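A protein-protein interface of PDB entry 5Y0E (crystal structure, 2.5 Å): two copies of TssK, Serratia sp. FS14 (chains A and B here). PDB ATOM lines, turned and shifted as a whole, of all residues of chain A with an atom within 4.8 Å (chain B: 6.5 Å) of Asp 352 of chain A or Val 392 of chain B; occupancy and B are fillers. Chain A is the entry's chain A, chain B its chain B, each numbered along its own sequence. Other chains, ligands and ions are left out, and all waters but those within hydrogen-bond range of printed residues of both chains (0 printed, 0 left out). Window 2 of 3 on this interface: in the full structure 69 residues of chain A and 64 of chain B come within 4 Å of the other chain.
The guanidinium group (NH2) of Arg 350 of chain A lies within hydrogen-bond range of the backbone carbonyl oxygen (O) of Gly 434 of chain A.
The backbone NH (N) of Asp 352 of chain A is in hydrogen-bond range of the backbone carbonyl oxygen (O) of Pro 433 of chain A (2.6 Å).
OD2 of Asp 352 of chain A is in salt-bridge range of NH1 of Arg 350 of chain A (2.9 Å).
Asp 352 of chain A touches just these residues of chain B: Pro 391 (3.5 Å), Val 392 (3.7 Å) and Arg 395 (3.9 Å).
Of the printed residues of chain A, Val 392 of chain B touches Ala 351 (3.6 Å), Asp 352 (3.7 Å) and Val 353 (3.8 Å).
Of the printed residues of chain B, Ala 351 of chain A touches Val 392 (3.6 Å).
Of the printed residues of chain B, Gly 434 of chain A touches Arg 395 (3.9 Å).
Of the printed residues of chain B, Arg 350 of chain A touches Arg 395 (3.3 Å).
Tyr 405 of chain B touches none of the printed residues of chain A.
The nearest residue of chain A that does not touch Val 392 of chain B is Arg 350 of chain A (4.5 Å).
The guanidinium group (NH2) of Arg 350 of chain A sits close to the guanidinium group (NE) of Arg 395 of chain B (3.3 Å).
No position is printed for both chains.
Of the 9 pairs that touch across the chains among the printed residues, none has its exchanged pair printed and touching as well.
Among the printed residues, pairs that only touch across the chains: Val 353 of chain A with Pro 391 of chain B, Asp 352 of chain A with Pro 391 of chain B, Ala 354 of chain A with Pro 391 of chain B, Ala 351 of chain A with Val 392 of chain B, Asp 352 of chain A with Val 392 of chain B, Val 353 of chain A with Val 392 of chain B, Gly 434 of chain A with Arg 395 of chain B and Asp 352 of chain A with Arg 395 of chain B.
Hydrophobic or aromatic side chains of chain B that line the printed part of chain A: Pro 391 and Val 392.
Printed residues of chain A that touch a printed residue of chain B: Arg 350, Ala 351, Asp 352, Val 353, Ala 354 and Gly 434.
Along chain A the printed residues that touch a printed residue of chain B span positions 350 to 434.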
ATOM      1  N   ARG A 350      -2.656 -27.230  12.474  1.00  0.00           N
ATOM      2  CA  ARG A 350      -3.943 -26.844  11.926  1.00  0.00           C
ATOM      3  C   ARG A 350      -4.399 -25.650  12.721  1.00  0.00           C
ATOM      4  O   ARG A 350      -4.137 -25.569  13.886  1.00  0.00           O
ATOM      5  CB  ARG A 350      -4.973 -27.954  12.009  1.00  0.00           C
ATOM      6  CG  ARG A 350      -6.102 -27.650  12.960  1.00  0.00           C
ATOM      7  CD  ARG A 350      -7.440 -28.126  12.469  1.00  0.00           C
ATOM      8  NE  ARG A 350      -8.389 -27.041  12.305  1.00  0.00           N
ATOM      9  CZ  ARG A 350      -8.566 -26.053  13.152  1.00  0.00           C
ATOM     10  NH1 ARG A 350      -9.442 -25.128  12.902  1.00  0.00           N
ATOM     11  NH2 ARG A 350      -7.865 -25.986  14.239  1.00  0.00           N
ATOM     12  N   ALA A 351      -5.054 -24.705  12.086  1.00  0.00           N
ATOM     13  CA  ALA A 351      -5.530 -23.533  12.776  1.00  0.00           C
ATOM     14  C   ALA A 351      -6.679 -22.929  12.029  1.00  0.00           C
ATOM     15  O   ALA A 351      -6.925 -23.272  10.912  1.00  0.00           O
ATOM     16  CB  ALA A 351      -4.424 -22.518  12.911  1.00  0.00           C
ATOM     17  N   ASP A 352      -7.378 -22.001  12.648  1.00  0.00           N
ATOM     18  CA  ASP A 352      -8.495 -21.383  11.982  1.00  0.00           C
ATOM     19  C   ASP A 352      -8.115 -20.119  11.262  1.00  0.00           C
ATOM     20  O   ASP A 352      -8.700 -19.093  11.456  1.00  0.00           O
ATOM     21  CB  ASP A 352      -9.615 -21.129  12.959  1.00  0.00           C
ATOM     22  CG  ASP A 352     -10.541 -22.287  13.077  1.00  0.00           C
ATOM     23  OD1 ASP A 352     -11.085 -22.684  12.068  1.00  0.00           O
ATOM     24  OD2 ASP A 352     -10.740 -22.824  14.162  1.00  0.00           O
ATOM     25  N   VAL A 353      -7.113 -20.211  10.422  1.00  0.00           N
ATOM     26  CA  VAL A 353      -6.686 -19.072   9.626  1.00  0.00           C
ATOM     27  C   VAL A 353      -6.773 -19.447   8.155  1.00  0.00           C
ATOM     28  O   VAL A 353      -7.125 -20.574   7.817  1.00  0.00           O
ATOM     29  CB  VAL A 353      -5.267 -18.639  10.010  1.00  0.00           C
ATOM     30  CG1 VAL A 353      -5.150 -18.573  11.506  1.00  0.00           C
ATOM     31  CG2 VAL A 353      -4.263 -19.607   9.454  1.00  0.00           C
ATOM     32  N   ALA A 354      -6.480 -18.514   7.266  1.00  0.00           N
ATOM     33  CA  ALA A 354      -6.472 -18.834   5.853  1.00  0.00           C
ATOM     34  C   ALA A 354      -5.212 -19.607   5.504  1.00  0.00           C
ATOM     35  O   ALA A 354      -4.150 -19.401   6.091  1.00  0.00           O
ATOM     36  CB  ALA A 354      -6.551 -17.571   5.005  1.00  0.00           C
ATOM     37  N   PRO A 433      -6.195 -18.524  15.940  1.00  0.00           N
ATOM     38  CA  PRO A 433      -7.347 -19.167  16.559  1.00  0.00           C
ATOM     39  C   PRO A 433      -7.444 -20.628  16.184  1.00  0.00           C
ATOM     40  O   PRO A 433      -7.239 -21.013  15.033  1.00  0.00           O
ATOM     41  CB  PRO A 433      -8.533 -18.375  15.999  1.00  0.00           C
ATOM     42  CG  PRO A 433      -8.011 -17.718  14.796  1.00  0.00           C
ATOM     43  CD  PRO A 433      -6.593 -17.406  15.081  1.00  0.00           C
ATOM     44  N   GLY A 434      -7.795 -21.440  17.167  1.00  0.00           N
ATOM     45  CA  GLY A 434      -8.047 -22.838  16.923  1.00  0.00           C
ATOM     46  C   GLY A 434      -6.819 -23.703  16.820  1.00  0.00           C
ATOM     47  O   GLY A 434      -6.953 -24.890  16.533  1.00  0.00           O
ATOM     48  N   THR B 389     -17.745 -16.053   4.791  1.00  0.00           N
ATOM     49  CA  THR B 389     -16.733 -16.983   4.403  1.00  0.00           C
ATOM     50  C   THR B 389     -15.804 -17.338   5.527  1.00  0.00           C
ATOM     51  O   THR B 389     -15.247 -16.491   6.141  1.00  0.00           O
ATOM     52  CB  THR B 389     -15.882 -16.400   3.294  1.00  0.00           C
ATOM     53  OG1 THR B 389     -16.697 -15.649   2.408  1.00  0.00           O
ATOM     54  CG2 THR B 389     -15.277 -17.471   2.540  1.00  0.00           C
ATOM     55  N   MET B 390     -15.632 -18.614   5.784  1.00  0.00           N
ATOM     56  CA  MET B 390     -14.746 -19.060   6.818  1.00  0.00           C
ATOM     57  C   MET B 390     -13.424 -19.331   6.187  1.00  0.00           C
ATOM     58  O   MET B 390     -13.363 -19.761   5.073  1.00  0.00           O
ATOM     59  CB  MET B 390     -15.301 -20.297   7.453  1.00  0.00           C
ATOM     60  CG  MET B 390     -16.726 -20.090   7.824  1.00  0.00           C
ATOM     61  SD  MET B 390     -17.462 -21.424   8.693  1.00  0.00           S
ATOM     62  CE  MET B 390     -16.311 -21.668   9.992  1.00  0.00           C
ATOM     63  N   PRO B 391     -12.350 -19.091   6.908  1.00  0.00           N
ATOM     64  CA  PRO B 391     -11.058 -19.284   6.255  1.00  0.00           C
ATOM     65  C   PRO B 391     -10.809 -20.732   5.939  1.00  0.00           C
ATOM     66  O   PRO B 391     -10.195 -21.047   4.916  1.00  0.00           O
ATOM     67  CB  PRO B 391     -10.069 -18.752   7.292  1.00  0.00           C
ATOM     68  CG  PRO B 391     -10.694 -19.088   8.559  1.00  0.00           C
ATOM     69  CD  PRO B 391     -12.191 -18.931   8.360  1.00  0.00           C
ATOM     70  N   VAL B 392     -11.319 -21.635   6.766  1.00  0.00           N
ATOM     71  CA  VAL B 392     -11.022 -23.045   6.621  1.00  0.00           C
ATOM     72  C   VAL B 392     -12.140 -23.806   7.296  1.00  0.00           C
ATOM     73  O   VAL B 392     -12.902 -23.245   8.076  1.00  0.00           O
ATOM     74  CB  VAL B 392      -9.641 -23.372   7.233  1.00  0.00           C
ATOM     75  CG1 VAL B 392      -9.776 -23.648   8.701  1.00  0.00           C
ATOM     76  CG2 VAL B 392      -9.019 -24.512   6.512  1.00  0.00           C
ATOM     77  N   ALA B 393     -12.262 -25.076   6.970  1.00  0.00           N
ATOM     78  CA  ALA B 393     -13.292 -25.881   7.588  1.00  0.00           C
ATOM     79  C   ALA B 393     -13.177 -25.764   9.099  1.00  0.00           C
ATOM     80  O   ALA B 393     -12.070 -25.857   9.636  1.00  0.00           O
ATOM     81  CB  ALA B 393     -13.171 -27.343   7.181  1.00  0.00           C
ATOM     82  N   PRO B 394     -14.272 -25.547   9.807  1.00  0.00           N
ATOM     83  CA  PRO B 394     -14.238 -25.680  11.254  1.00  0.00           C
ATOM     84  C   PRO B 394     -13.763 -27.068  11.627  1.00  0.00           C
ATOM     85  O   PRO B 394     -13.634 -27.967  10.804  1.00  0.00           O
ATOM     86  CB  PRO B 394     -15.691 -25.470  11.681  1.00  0.00           C
ATOM     87  CG  PRO B 394     -16.406 -25.063  10.481  1.00  0.00           C
ATOM     88  CD  PRO B 394     -15.642 -25.478   9.297  1.00  0.00           C
ATOM     89  N   ARG B 395     -13.541 -27.243  12.905  1.00  0.00           N
ATOM     90  CA  ARG B 395     -12.939 -28.450  13.410  1.00  0.00           C
ATOM     91  C   ARG B 395     -13.972 -29.478  13.770  1.00  0.00           C
ATOM     92  O   ARG B 395     -13.644 -30.658  13.887  1.00  0.00           O
ATOM     93  CB  ARG B 395     -12.131 -28.103  14.644  1.00  0.00           C
ATOM     94  CG  ARG B 395     -11.809 -26.638  14.664  1.00  0.00           C
ATOM     95  CD  ARG B 395     -11.321 -26.201  16.031  1.00  0.00           C
ATOM     96  NE  ARG B 395     -10.184 -27.017  16.410  1.00  0.00           N
ATOM     97  CZ  ARG B 395      -9.854 -27.260  17.670  1.00  0.00           C
ATOM     98  NH1 ARG B 395     -10.588 -26.759  18.657  1.00  0.00           N
ATOM     99  NH2 ARG B 395      -8.798 -28.007  17.940  1.00  0.00           N
ATOM    100  N   TYR B 399     -13.013 -32.403   7.344  1.00  0.00           N
ATOM    101  CA  TYR B 399     -12.389 -31.715   6.228  1.00  0.00           C
ATOM    102  C   TYR B 399     -12.747 -32.385   4.905  1.00  0.00           C
ATOM    103  O   TYR B 399     -12.656 -33.606   4.769  1.00  0.00           O
ATOM    104  CB  TYR B 399     -10.882 -31.721   6.420  1.00  0.00           C
ATOM    105  CG  TYR B 399     -10.082 -31.035   5.344  1.00  0.00           C
ATOM    106  CD1 TYR B 399     -10.031 -29.662   5.270  1.00  0.00           C
ATOM    107  CD2 TYR B 399      -9.332 -31.762   4.437  1.00  0.00           C
ATOM    108  CE1 TYR B 399      -9.282 -29.031   4.318  1.00  0.00           C
ATOM    109  CE2 TYR B 399      -8.569 -31.130   3.475  1.00  0.00           C
ATOM    110  CZ  TYR B 399      -8.556 -29.761   3.429  1.00  0.00           C
ATOM    111  OH  TYR B 399      -7.820 -29.104   2.486  1.00  0.00           O
ATOM    112  N   TYR B 405     -16.406 -22.995   2.938  1.00  0.00           N
ATOM    113  CA  TYR B 405     -17.301 -22.926   4.057  1.00  0.00           C
ATOM    114  C   TYR B 405     -17.854 -21.551   4.323  1.00  0.00           C
ATOM    115  O   TYR B 405     -17.153 -20.603   4.311  1.00  0.00           O
ATOM    116  CB  TYR B 405     -16.574 -23.494   5.261  1.00  0.00           C
ATOM    117  CG  TYR B 405     -16.173 -24.923   5.040  1.00  0.00           C
ATOM    118  CD1 TYR B 405     -15.074 -25.239   4.300  1.00  0.00           C
ATOM    119  CD2 TYR B 405     -16.929 -25.946   5.529  1.00  0.00           C
ATOM    120  CE1 TYR B 405     -14.734 -26.533   4.072  1.00  0.00           C
ATOM    121  CE2 TYR B 405     -16.586 -27.238   5.312  1.00  0.00           C
ATOM    122  CZ  TYR B 405     -15.485 -27.517   4.580  1.00  0.00           C
ATOM    123  OH  TYR B 405     -15.140 -28.796   4.360  1.00  0.00           O
